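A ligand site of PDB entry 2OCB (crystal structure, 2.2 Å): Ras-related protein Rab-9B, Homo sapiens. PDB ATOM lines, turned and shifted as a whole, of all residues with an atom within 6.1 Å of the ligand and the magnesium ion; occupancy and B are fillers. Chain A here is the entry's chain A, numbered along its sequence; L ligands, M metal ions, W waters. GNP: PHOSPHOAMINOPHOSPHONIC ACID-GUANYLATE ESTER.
The backbone NH of Ser 21 lies close to an oxygen (O2B) of the ligand.
N of Thr 39 lies close to O2G of the ligand (2.7 Å).
The side-chain amino group of Lys 125 lies within hydrogen-bond range of an oxygen (O4') of the ligand, at 2.6 Å.
The backbone NH (N) of Ser 22 is in hydrogen-bond range of an oxygen (O1A) of the ligand (3.0 Å).
An oxygen (O1A) of the ligand sits at hydrogen-bond distance from the side-chain hydroxyl (OG) of Ser 22 (2.6 Å).
The backbone carbonyl oxygen (O) of Asp 33 sits at hydrogen-bond distance from an oxygen (O2') of the ligand (2.6 Å).
A ring nitrogen (ND1) of His 38 is in hydrogen-bond range of an oxygen (O1G) of the ligand, at 2.7 Å.
O of Ser 34 sits at hydrogen-bond distance from O3' of the ligand (2.7 Å).
The backbone NH (N) of Lys 20 is in hydrogen-bond range of an oxygen (O1B) of the ligand, at 3.2 Å.
The side-chain amino group (NZ) of Lys 20 is in salt-bridge range of an oxygen (O3G) of the ligand (2.7 Å).
The backbone NH (N) of Gly 65 lies within hydrogen-bond range of an oxygen (O3G) of the ligand (2.8 Å).
OD2 of Asp 127 lies within hydrogen-bond range of N2 of the ligand (2.9 Å).
The backbone NH (N) of Ala 155 sits at hydrogen-bond distance from an oxygen (O6) of the ligand (2.9 Å).
O1B of the ligand lies within hydrogen-bond range of N of Gly 19.
The side-chain amide nitrogen (ND2) of Asn 124 lies within hydrogen-bond range of a nitrogen (N7) of the ligand (3.2 Å).
O1B of the ligand lies within hydrogen-bond range of N of Val 18 (3.2 Å).
The backbone NH (N) of Lys 156 sits at hydrogen-bond distance from an oxygen (O6) of the ligand (3.3 Å).
Residues that only touch the magnesium ion: Asp 62.
Of the 34 residues printed, 3 come within 4 Å of the magnesium ion.
Water W2 bridges the side-chain carboxylate (OD1) of Asp 62 (2.5 Å) and the backbone carbonyl oxygen (O) of Thr 63 (2.6 Å).
Water W3 bridges the backbone carbonyl oxygen of Phe 37 and an oxygen (O2A) of the ligand.
Water W1 lies within hydrogen-bond range of an oxygen (O2A) of the ligand and the backbone NH (N) of His 38.
Water W5 lies within hydrogen-bond range of the side-chain amino group (NZ) of Lys 125, the side-chain amino group (NZ) of Lys 128 and a nitrogen (N3) of the ligand.
Water W4 lies within hydrogen-bond range of O of Thr 39 (2.6 Å), NE2 of Gln 66 (2.9 Å), O1G of the ligand (3.1 Å) and N of Gly 65 (3.4 Å).
The backbone NH of Gly 17 lies close to a nitrogen (N3B) of the ligand (3.2 Å).
Residues that only touch the ligand: Lys 128 (3.1 Å), Ala 36 (3.2 Å), Ser 154 (3.2 Å), Phe 32 (3.4 Å), Gly 16 (3.5 Å), Ala 64 (3.8 Å), Thr 63 (3.9 Å) and Asp 15 (3.9 Å).
Hydrophobic or aromatic side chains that line the ligand: Val 18, Phe 32, Ala 36, His 38 and Ala 155.
Of the 34 residues printed, 24 come within 4 Å of the ligand.
The nearest printed residue that does not touch the ligand is Gln 35 (4.2 Å).
The backbone carbonyl oxygen of Thr 153 is in hydrogen-bond range of the backbone NH of Lys 125 (3.0 Å).
The backbone NH (N) of Gln 35 lies within hydrogen-bond range of the side-chain carboxylate (OD1) of Asp 33 (2.6 Å).
The side-chain amide nitrogen (NE2) of Gln 66 lies within hydrogen-bond range of a ring nitrogen (ND1) of His 38 (3.5 Å).
The backbone carbonyl oxygen (O) of Asp 15 is in hydrogen-bond range of the side-chain amino group (NZ) of Lys 20.
The side-chain carboxylate (OD1) of Asp 127 lies within hydrogen-bond range of the side-chain hydroxyl (OG) of Ser 154, 2.6 Å away.
OD1 of Asn 124 is in hydrogen-bond range of N of Ala 155 (3.3 Å).
The side-chain hydroxyl (OG) of Ser 154 lies close to the backbone NH (N) of Lys 156, 3.2 Å away.
The side-chain hydroxyl of Ser 154 lies within hydrogen-bond range of the backbone NH of Asp 157 (2.7 Å).
The magnesium ion is bound by water W3 (2.1 Å), an oxygen (O2B) of the ligand (2.1 Å), the side-chain hydroxyl (OG) of Ser 21 (2.1 Å), an oxygen (O2G) of the ligand (2.2 Å), the side-chain hydroxyl (OG1) of Thr 39 (2.2 Å) and water W2 (2.3 Å).
The magnesium ion has six donor atoms within binding distance.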
ATOM      1  N   GLY A  14     -16.014  21.298 -13.698  1.00  0.00           N
ATOM      2  CA  GLY A  14     -15.923  20.168 -14.603  1.00  0.00           C
ATOM      3  C   GLY A  14     -15.628  20.624 -15.998  1.00  0.00           C
ATOM      4  O   GLY A  14     -15.717  21.808 -16.304  1.00  0.00           O
ATOM      5  N   ASP A  15     -15.251  19.674 -16.856  1.00  0.00           N
ATOM      6  CA  ASP A  15     -14.856  19.970 -18.239  1.00  0.00           C
ATOM      7  C   ASP A  15     -15.918  20.747 -19.009  1.00  0.00           C
ATOM      8  O   ASP A  15     -17.122  20.660 -18.706  1.00  0.00           O
ATOM      9  CB  ASP A  15     -14.524  18.694 -18.997  1.00  0.00           C
ATOM     10  CG  ASP A  15     -13.180  18.114 -18.607  1.00  0.00           C
ATOM     11  OD1 ASP A  15     -12.529  18.559 -17.622  1.00  0.00           O
ATOM     12  OD2 ASP A  15     -12.783  17.192 -19.310  1.00  0.00           O
ATOM     13  N   GLY A  16     -15.456  21.536 -19.975  1.00  0.00           N
ATOM     14  CA  GLY A  16     -16.331  22.235 -20.908  1.00  0.00           C
ATOM     15  C   GLY A  16     -17.341  21.264 -21.494  1.00  0.00           C
ATOM     16  O   GLY A  16     -16.991  20.144 -21.834  1.00  0.00           O
ATOM     17  N   GLY A  17     -18.586  21.675 -21.573  1.00  0.00           N
ATOM     18  CA  GLY A  17     -19.633  20.877 -22.234  1.00  0.00           C
ATOM     19  C   GLY A  17     -20.443  19.901 -21.362  1.00  0.00           C
ATOM     20  O   GLY A  17     -21.410  19.326 -21.837  1.00  0.00           O
ATOM     21  N   VAL A  18     -20.065  19.748 -20.087  1.00  0.00           N
ATOM     22  CA  VAL A  18     -20.618  18.667 -19.246  1.00  0.00           C
ATOM     23  C   VAL A  18     -22.071  18.937 -18.797  1.00  0.00           C
ATOM     24  O   VAL A  18     -22.813  17.993 -18.526  1.00  0.00           O
ATOM     25  CB  VAL A  18     -19.679  18.320 -17.987  1.00  0.00           C
ATOM     26  CG1 VAL A  18     -18.334  17.817 -18.457  1.00  0.00           C
ATOM     27  CG2 VAL A  18     -19.541  19.505 -16.987  1.00  0.00           C
ATOM     28  N   GLY A  19     -22.460  20.202 -18.717  1.00  0.00           N
ATOM     29  CA  GLY A  19     -23.804  20.601 -18.335  1.00  0.00           C
ATOM     30  C   GLY A  19     -23.906  21.434 -17.064  1.00  0.00           C
ATOM     31  O   GLY A  19     -24.993  21.601 -16.566  1.00  0.00           O
ATOM     32  N   LYS A  20     -22.800  21.998 -16.571  1.00  0.00           N
ATOM     33  CA  LYS A  20     -22.806  22.778 -15.317  1.00  0.00           C
ATOM     34  C   LYS A  20     -23.790  23.925 -15.272  1.00  0.00           C
ATOM     35  O   LYS A  20     -24.543  24.073 -14.290  1.00  0.00           O
ATOM     36  CB  LYS A  20     -21.413  23.326 -14.993  1.00  0.00           C
ATOM     37  CG  LYS A  20     -20.304  22.285 -14.899  1.00  0.00           C
ATOM     38  CD  LYS A  20     -18.980  22.904 -14.577  1.00  0.00           C
ATOM     39  CE  LYS A  20     -18.400  23.764 -15.700  1.00  0.00           C
ATOM     40  NZ  LYS A  20     -18.193  23.004 -16.973  1.00  0.00           N
ATOM     41  N   SER A  21     -23.751  24.786 -16.286  1.00  0.00           N
ATOM     42  CA  SER A  21     -24.668  25.917 -16.349  1.00  0.00           C
ATOM     43  C   SER A  21     -26.111  25.487 -16.588  1.00  0.00           C
ATOM     44  O   SER A  21     -27.022  26.074 -16.047  1.00  0.00           O
ATOM     45  CB  SER A  21     -24.272  26.863 -17.490  1.00  0.00           C
ATOM     46  OG  SER A  21     -22.914  27.160 -17.413  1.00  0.00           O
ATOM     47  N   SER A  22     -26.293  24.487 -17.410  1.00  0.00           N
ATOM     48  CA  SER A  22     -27.607  23.851 -17.598  1.00  0.00           C
ATOM     49  C   SER A  22     -28.132  23.266 -16.318  1.00  0.00           C
ATOM     50  O   SER A  22     -29.321  23.401 -16.004  1.00  0.00           O
ATOM     51  CB  SER A  22     -27.513  22.740 -18.631  1.00  0.00           C
ATOM     52  OG  SER A  22     -27.165  23.282 -19.878  1.00  0.00           O
ATOM     53  N   LEU A  23     -27.260  22.633 -15.535  1.00  0.00           N
ATOM     54  CA  LEU A  23     -27.661  22.124 -14.205  1.00  0.00           C
ATOM     55  C   LEU A  23     -28.118  23.255 -13.273  1.00  0.00           C
ATOM     56  O   LEU A  23     -29.186  23.142 -12.663  1.00  0.00           O
ATOM     57  CB  LEU A  23     -26.520  21.336 -13.548  1.00  0.00           C
ATOM     58  CG  LEU A  23     -26.315  19.906 -13.952  1.00  0.00           C
ATOM     59  CD1 LEU A  23     -24.982  19.370 -13.359  1.00  0.00           C
ATOM     60  CD2 LEU A  23     -27.577  19.075 -13.519  1.00  0.00           C
ATOM     61  N   PHE A  32     -34.264  25.139 -19.515  1.00  0.00           N
ATOM     62  CA  PHE A  32     -33.195  24.404 -20.231  1.00  0.00           C
ATOM     63  C   PHE A  32     -33.028  24.960 -21.671  1.00  0.00           C
ATOM     64  O   PHE A  32     -34.000  25.070 -22.424  1.00  0.00           O
ATOM     65  CB  PHE A  32     -33.526  22.930 -20.341  1.00  0.00           C
ATOM     66  CG  PHE A  32     -32.462  22.093 -21.027  1.00  0.00           C
ATOM     67  CD1 PHE A  32     -31.283  21.780 -20.392  1.00  0.00           C
ATOM     68  CD2 PHE A  32     -32.676  21.582 -22.299  1.00  0.00           C
ATOM     69  CE1 PHE A  32     -30.331  20.997 -21.010  1.00  0.00           C
ATOM     70  CE2 PHE A  32     -31.717  20.791 -22.927  1.00  0.00           C
ATOM     71  CZ  PHE A  32     -30.562  20.494 -22.280  1.00  0.00           C
ATOM     72  N   ASP A  33     -31.786  25.292 -22.030  1.00  0.00           N
ATOM     73  CA  ASP A  33     -31.406  25.650 -23.380  1.00  0.00           C
ATOM     74  C   ASP A  33     -30.641  24.503 -24.055  1.00  0.00           C
ATOM     75  O   ASP A  33     -29.548  24.089 -23.609  1.00  0.00           O
ATOM     76  CB  ASP A  33     -30.526  26.887 -23.321  1.00  0.00           C
ATOM     77  CG  ASP A  33     -30.361  27.567 -24.659  1.00  0.00           C
ATOM     78  OD1 ASP A  33     -30.199  26.871 -25.715  1.00  0.00           O
ATOM     79  OD2 ASP A  33     -30.338  28.819 -24.638  1.00  0.00           O
ATOM     80  N   SER A  34     -31.208  24.002 -25.145  1.00  0.00           N
ATOM     81  CA  SER A  34     -30.548  22.995 -25.985  1.00  0.00           C
ATOM     82  C   SER A  34     -29.236  23.488 -26.660  1.00  0.00           C
ATOM     83  O   SER A  34     -28.343  22.679 -26.976  1.00  0.00           O
ATOM     84  CB  SER A  34     -31.542  22.534 -27.060  1.00  0.00           C
ATOM     85  OG  SER A  34     -30.921  21.602 -27.937  1.00  0.00           O
ATOM     86  N   GLN A  35     -29.136  24.795 -26.904  1.00  0.00           N
ATOM     87  CA  GLN A  35     -27.979  25.392 -27.592  1.00  0.00           C
ATOM     88  C   GLN A  35     -27.208  26.299 -26.625  1.00  0.00           C
ATOM     89  O   GLN A  35     -27.119  27.541 -26.820  1.00  0.00           O
ATOM     90  CB  GLN A  35     -28.437  26.171 -28.845  1.00  0.00           C
ATOM     91  N   ALA A  36     -26.658  25.703 -25.578  1.00  0.00           N
ATOM     92  CA  ALA A  36     -26.009  26.489 -24.497  1.00  0.00           C
ATOM     93  C   ALA A  36     -24.568  26.837 -24.883  1.00  0.00           C
ATOM     94  O   ALA A  36     -23.813  26.011 -25.461  1.00  0.00           O
ATOM     95  CB  ALA A  36     -26.054  25.757 -23.160  1.00  0.00           C
ATOM     96  N   PHE A  37     -24.196  28.084 -24.566  1.00  0.00           N
ATOM     97  CA  PHE A  37     -22.929  28.658 -24.998  1.00  0.00           C
ATOM     98  C   PHE A  37     -21.935  28.564 -23.851  1.00  0.00           C
ATOM     99  O   PHE A  37     -22.281  28.801 -22.687  1.00  0.00           O
ATOM    100  CB  PHE A  37     -23.150  30.116 -25.423  1.00  0.00           C
ATOM    101  CG  PHE A  37     -24.370  30.317 -26.281  1.00  0.00           C
ATOM    102  CD1 PHE A  37     -24.299  30.191 -27.668  1.00  0.00           C
ATOM    103  CD2 PHE A  37     -25.621  30.585 -25.687  1.00  0.00           C
ATOM    104  CE1 PHE A  37     -25.433  30.343 -28.459  1.00  0.00           C
ATOM    105  CE2 PHE A  37     -26.776  30.740 -26.484  1.00  0.00           C
ATOM    106  CZ  PHE A  37     -26.679  30.628 -27.875  1.00  0.00           C
ATOM    107  N   HIS A  38     -20.701  28.202 -24.192  1.00  0.00           N
ATOM    108  CA  HIS A  38     -19.602  28.154 -23.232  1.00  0.00           C
ATOM    109  C   HIS A  38     -19.587  29.345 -22.289  1.00  0.00           C
ATOM    110  O   HIS A  38     -19.855  30.487 -22.678  1.00  0.00           O
ATOM    111  CB  HIS A  38     -18.265  28.030 -23.963  1.00  0.00           C
ATOM    112  CG  HIS A  38     -18.070  26.713 -24.643  1.00  0.00           C
ATOM    113  ND1 HIS A  38     -17.756  25.561 -23.949  1.00  0.00           N
ATOM    114  CD2 HIS A  38     -18.213  26.351 -25.933  1.00  0.00           C
ATOM    115  CE1 HIS A  38     -17.675  24.547 -24.792  1.00  0.00           C
ATOM    116  NE2 HIS A  38     -17.957  24.999 -26.007  1.00  0.00           N
ATOM    117  N   THR A  39     -19.362  29.027 -21.007  1.00  0.00           N
ATOM    118  CA  THR A  39     -19.133  30.049 -19.965  1.00  0.00           C
ATOM    119  C   THR A  39     -17.674  30.476 -20.117  1.00  0.00           C
ATOM    120  O   THR A  39     -16.801  29.631 -20.384  1.00  0.00           O
ATOM    121  CB  THR A  39     -19.452  29.454 -18.572  1.00  0.00           C
ATOM    122  OG1 THR A  39     -20.777  28.938 -18.631  1.00  0.00           O
ATOM    123  CG2 THR A  39     -19.372  30.489 -17.372  1.00  0.00           C
ATOM    124  N   ILE A  40     -17.422  31.791 -20.029  1.00  0.00           N
ATOM    125  CA  ILE A  40     -16.060  32.308 -20.205  1.00  0.00           C
ATOM    126  C   ILE A  40     -15.424  32.811 -18.917  1.00  0.00           C
ATOM    127  O   ILE A  40     -14.245  33.133 -18.875  1.00  0.00           O
ATOM    128  CB  ILE A  40     -15.948  33.407 -21.330  1.00  0.00           C
ATOM    129  CG1 ILE A  40     -16.717  34.666 -20.969  1.00  0.00           C
ATOM    130  CG2 ILE A  40     -16.389  32.848 -22.702  1.00  0.00           C
ATOM    131  CD1 ILE A  40     -16.631  35.727 -22.090  1.00  0.00           C
ATOM    132  N   ASP A  62     -21.205  29.141 -10.902  1.00  0.00           N
ATOM    133  CA  ASP A  62     -20.929  28.474 -12.186  1.00  0.00           C
ATOM    134  C   ASP A  62     -19.549  28.941 -12.671  1.00  0.00           C
ATOM    135  O   ASP A  62     -19.170  30.079 -12.465  1.00  0.00           O
ATOM    136  CB  ASP A  62     -22.028  28.832 -13.199  1.00  0.00           C
ATOM    137  CG  ASP A  62     -21.962  27.997 -14.491  1.00  0.00           C
ATOM    138  OD1 ASP A  62     -21.382  26.912 -14.493  1.00  0.00           O
ATOM    139  OD2 ASP A  62     -22.473  28.443 -15.521  1.00  0.00           O
ATOM    140  N   THR A  63     -18.797  28.043 -13.304  1.00  0.00           N
ATOM    141  CA  THR A  63     -17.461  28.360 -13.816  1.00  0.00           C
ATOM    142  C   THR A  63     -17.267  27.866 -15.278  1.00  0.00           C
ATOM    143  O   THR A  63     -17.950  26.947 -15.765  1.00  0.00           O
ATOM    144  CB  THR A  63     -16.374  27.721 -12.948  1.00  0.00           C
ATOM    145  OG1 THR A  63     -16.438  26.287 -13.049  1.00  0.00           O
ATOM    146  CG2 THR A  63     -16.516  28.128 -11.481  1.00  0.00           C
ATOM    147  N   ALA A  64     -16.359  28.523 -15.984  1.00  0.00           N
ATOM    148  CA  ALA A  64     -15.868  28.043 -17.284  1.00  0.00           C
ATOM    149  C   ALA A  64     -15.088  26.729 -17.117  1.00  0.00           C
ATOM    150  O   ALA A  64     -14.119  26.675 -16.393  1.00  0.00           O
ATOM    151  CB  ALA A  64     -14.946  29.106 -17.898  1.00  0.00           C
ATOM    152  N   GLY A  65     -15.513  25.681 -17.811  1.00  0.00           N
ATOM    153  CA  GLY A  65     -14.880  24.409 -17.734  1.00  0.00           C
ATOM    154  C   GLY A  65     -13.609  24.345 -18.579  1.00  0.00           C
ATOM    155  O   GLY A  65     -12.762  23.521 -18.334  1.00  0.00           O
ATOM    156  N   GLN A  66     -13.504  25.229 -19.581  1.00  0.00           N
ATOM    157  CA  GLN A  66     -12.366  25.261 -20.501  1.00  0.00           C
ATOM    158  C   GLN A  66     -11.082  25.787 -19.837  1.00  0.00           C
ATOM    159  O   GLN A  66     -11.113  26.785 -19.072  1.00  0.00           O
ATOM    160  CB  GLN A  66     -12.702  26.091 -21.726  1.00  0.00           C
ATOM    161  CG  GLN A  66     -13.769  25.472 -22.602  1.00  0.00           C
ATOM    162  CD  GLN A  66     -14.125  26.350 -23.799  1.00  0.00           C
ATOM    163  OE1 GLN A  66     -13.755  26.054 -24.929  1.00  0.00           O
ATOM    164  NE2 GLN A  66     -14.858  27.413 -23.560  1.00  0.00           N
ATOM    165  N   ASN A 124     -23.706  13.873 -15.377  1.00  0.00           N
ATOM    166  CA  ASN A 124     -24.825  14.494 -16.095  1.00  0.00           C
ATOM    167  C   ASN A 124     -25.087  13.840 -17.466  1.00  0.00           C
ATOM    168  O   ASN A 124     -24.259  13.080 -17.938  1.00  0.00           O
ATOM    169  CB  ASN A 124     -24.562  15.989 -16.244  1.00  0.00           C
ATOM    170  CG  ASN A 124     -25.809  16.778 -16.620  1.00  0.00           C
ATOM    171  OD1 ASN A 124     -26.882  16.503 -16.136  1.00  0.00           O
ATOM    172  ND2 ASN A 124     -25.657  17.764 -17.490  1.00  0.00           N
ATOM    173  N   LYS A 125     -26.228  14.184 -18.071  1.00  0.00           N
ATOM    174  CA  LYS A 125     -26.605  13.775 -19.423  1.00  0.00           C
ATOM    175  C   LYS A 125     -27.020  12.304 -19.436  1.00  0.00           C
ATOM    176  O   LYS A 125     -26.651  11.562 -20.338  1.00  0.00           O
ATOM    177  CB  LYS A 125     -25.461  14.018 -20.453  1.00  0.00           C
ATOM    178  CG  LYS A 125     -24.883  15.431 -20.430  1.00  0.00           C
ATOM    179  CD  LYS A 125     -24.413  15.877 -21.785  1.00  0.00           C
ATOM    180  CE  LYS A 125     -23.740  17.213 -21.696  1.00  0.00           C
ATOM    181  NZ  LYS A 125     -23.733  17.994 -22.975  1.00  0.00           N
ATOM    182  N   VAL A 126     -27.785  11.904 -18.417  1.00  0.00           N
ATOM    183  CA  VAL A 126     -28.118  10.489 -18.216  1.00  0.00           C
ATOM    184  C   VAL A 126     -29.222  10.079 -19.209  1.00  0.00           C
ATOM    185  O   VAL A 126     -29.294   8.936 -19.632  1.00  0.00           O
ATOM    186  CB  VAL A 126     -28.500  10.188 -16.718  1.00  0.00           C
ATOM    187  CG1 VAL A 126     -29.939  10.618 -16.414  1.00  0.00           C
ATOM    188  CG2 VAL A 126     -28.294   8.723 -16.389  1.00  0.00           C
ATOM    189  N   ASP A 127     -30.045  11.056 -19.588  1.00  0.00           N
ATOM    190  CA  ASP A 127     -31.056  10.951 -20.651  1.00  0.00           C
ATOM    191  C   ASP A 127     -30.537  10.537 -22.028  1.00  0.00           C
ATOM    192  O   ASP A 127     -31.290   9.997 -22.826  1.00  0.00           O
ATOM    193  CB  ASP A 127     -31.797  12.275 -20.800  1.00  0.00           C
ATOM    194  CG  ASP A 127     -30.874  13.446 -21.142  1.00  0.00           C
ATOM    195  OD1 ASP A 127     -30.427  14.152 -20.199  1.00  0.00           O
ATOM    196  OD2 ASP A 127     -30.591  13.655 -22.349  1.00  0.00           O
ATOM    197  N   LYS A 128     -29.264  10.787 -22.308  1.00  0.00           N
ATOM    198  CA  LYS A 128     -28.680  10.487 -23.624  1.00  0.00           C
ATOM    199  C   LYS A 128     -28.388   9.004 -23.772  1.00  0.00           C
ATOM    200  O   LYS A 128     -28.037   8.338 -22.787  1.00  0.00           O
ATOM    201  CB  LYS A 128     -27.412  11.325 -23.864  1.00  0.00           C
ATOM    202  CG  LYS A 128     -27.705  12.836 -23.988  1.00  0.00           C
ATOM    203  CD  LYS A 128     -26.450  13.679 -24.167  1.00  0.00           C
ATOM    204  CE  LYS A 128     -25.992  13.751 -25.620  1.00  0.00           C
ATOM    205  NZ  LYS A 128     -24.891  14.752 -25.806  1.00  0.00           N
ATOM    206  N   THR A 153     -27.563  12.664 -13.329  1.00  0.00           N
ATOM    207  CA  THR A 153     -28.417  13.816 -13.482  1.00  0.00           C
ATOM    208  C   THR A 153     -28.747  14.037 -14.937  1.00  0.00           C
ATOM    209  O   THR A 153     -28.074  13.535 -15.841  1.00  0.00           O
ATOM    210  CB  THR A 153     -27.779  15.116 -12.859  1.00  0.00           C
ATOM    211  OG1 THR A 153     -26.506  15.384 -13.464  1.00  0.00           O
ATOM    212  CG2 THR A 153     -27.554  14.952 -11.386  1.00  0.00           C
ATOM    213  N   SER A 154     -29.810  14.754 -15.173  1.00  0.00           N
ATOM    214  CA  SER A 154     -30.029  15.305 -16.471  1.00  0.00           C
ATOM    215  C   SER A 154     -30.688  16.622 -16.293  1.00  0.00           C
ATOM    216  O   SER A 154     -31.855  16.661 -15.926  1.00  0.00           O
ATOM    217  CB  SER A 154     -30.934  14.411 -17.330  1.00  0.00           C
ATOM    218  OG  SER A 154     -31.718  15.188 -18.228  1.00  0.00           O
ATOM    219  N   ALA A 155     -29.925  17.694 -16.543  1.00  0.00           N
ATOM    220  CA  ALA A 155     -30.465  19.059 -16.698  1.00  0.00           C
ATOM    221  C   ALA A 155     -31.618  19.113 -17.678  1.00  0.00           C
ATOM    222  O   ALA A 155     -32.589  19.843 -17.471  1.00  0.00           O
ATOM    223  CB  ALA A 155     -29.371  20.021 -17.165  1.00  0.00           C
ATOM    224  N   LYS A 156     -31.501  18.337 -18.749  1.00  0.00           N
ATOM    225  CA  LYS A 156     -32.489  18.322 -19.830  1.00  0.00           C
ATOM    226  C   LYS A 156     -33.859  17.856 -19.361  1.00  0.00           C
ATOM    227  O   LYS A 156     -34.867  18.543 -19.576  1.00  0.00           O
ATOM    228  CB  LYS A 156     -32.012  17.441 -20.979  1.00  0.00           C
ATOM    229  CG  LYS A 156     -32.986  17.401 -22.134  1.00  0.00           C
ATOM    230  CD  LYS A 156     -32.485  16.610 -23.301  1.00  0.00           C
ATOM    231  CE  LYS A 156     -33.602  16.512 -24.367  1.00  0.00           C
ATOM    232  NZ  LYS A 156     -33.054  16.292 -25.713  1.00  0.00           N
ATOM    233  N   ASP A 157     -33.901  16.677 -18.722  1.00  0.00           N
ATOM    234  CA  ASP A 157     -35.144  16.065 -18.243  1.00  0.00           C
ATOM    235  C   ASP A 157     -35.535  16.428 -16.800  1.00  0.00           C
ATOM    236  O   ASP A 157     -36.650  16.143 -16.355  1.00  0.00           O
ATOM    237  CB  ASP A 157     -35.065  14.545 -18.406  1.00  0.00           C
ATOM    238  CG  ASP A 157     -35.052  14.109 -19.850  1.00  0.00           C
ATOM    239  OD1 ASP A 157     -35.484  14.913 -20.715  1.00  0.00           O
ATOM    240  OD2 ASP A 157     -34.623  12.980 -20.142  1.00  0.00           O
HETATM  241  PG  GNP L   1     -18.779  25.341 -20.079  1.00  0.00           P
HETATM  242  O1G GNP L   1     -17.867  25.358 -21.280  1.00  0.00           O
HETATM  243  O2G GNP L   1     -19.431  26.627 -19.829  1.00  0.00           O
HETATM  244  O3G GNP L   1     -17.852  24.830 -18.990  1.00  0.00           O
HETATM  245  N3B GNP L   1     -19.974  24.290 -20.399  1.00  0.00           N
HETATM  246  PB  GNP L   1     -21.122  23.686 -19.441  1.00  0.00           P
HETATM  247  O1B GNP L   1     -20.447  22.621 -18.652  1.00  0.00           O
HETATM  248  O2B GNP L   1     -21.751  24.759 -18.656  1.00  0.00           O
HETATM  249  O3A GNP L   1     -22.235  23.033 -20.319  1.00  0.00           O
HETATM  250  PA  GNP L   1     -23.588  23.599 -20.815  1.00  0.00           P
HETATM  251  O1A GNP L   1     -24.605  23.799 -19.772  1.00  0.00           O
HETATM  252  O2A GNP L   1     -23.367  24.822 -21.642  1.00  0.00           O
HETATM  253  O5' GNP L   1     -24.202  22.531 -21.740  1.00  0.00           O
HETATM  254  C5' GNP L   1     -23.491  22.006 -22.879  1.00  0.00           C
HETATM  255  C4' GNP L   1     -24.450  21.409 -23.919  1.00  0.00           C
HETATM  256  O4' GNP L   1     -25.023  20.183 -23.383  1.00  0.00           O
HETATM  257  C3' GNP L   1     -25.657  22.264 -24.365  1.00  0.00           C
HETATM  258  O3' GNP L   1     -26.012  22.060 -25.770  1.00  0.00           O
HETATM  259  C2' GNP L   1     -26.792  21.790 -23.466  1.00  0.00           C
HETATM  260  O2' GNP L   1     -28.080  21.957 -24.060  1.00  0.00           O
HETATM  261  C1' GNP L   1     -26.426  20.313 -23.289  1.00  0.00           C
HETATM  262  N9  GNP L   1     -26.844  19.720 -22.005  1.00  0.00           N
HETATM  263  C8  GNP L   1     -26.675  20.196 -20.712  1.00  0.00           C
HETATM  264  N7  GNP L   1     -27.175  19.385 -19.804  1.00  0.00           N
HETATM  265  C5  GNP L   1     -27.702  18.316 -20.547  1.00  0.00           C
HETATM  266  C6  GNP L   1     -28.370  17.115 -20.158  1.00  0.00           C
HETATM  267  O6  GNP L   1     -28.676  16.740 -19.034  1.00  0.00           O
HETATM  268  N1  GNP L   1     -28.720  16.321 -21.252  1.00  0.00           N
HETATM  269  C2  GNP L   1     -28.461  16.616 -22.589  1.00  0.00           C
HETATM  270  N2  GNP L   1     -28.864  15.720 -23.519  1.00  0.00           N
HETATM  271  N3  GNP L   1     -27.831  17.717 -22.961  1.00  0.00           N
HETATM  272  C4  GNP L   1     -27.494  18.519 -21.902  1.00  0.00           C
HETATM  273 MG    MG M   1     -21.288  26.839 -18.760  1.00  0.00          MG
HETATM  274  O   HOH W   1     -21.107  24.970 -23.098  1.00  0.00           O
HETATM  275  O   HOH W   2     -20.291  26.647 -16.745  1.00  0.00           O
HETATM  276  O   HOH W   3     -22.536  27.318 -20.405  1.00  0.00           O
HETATM  277  O   HOH W   4     -15.600  27.368 -20.716  1.00  0.00           O
HETATM  278  O   HOH W   5     -25.549  17.308 -24.949  1.00  0.00           O
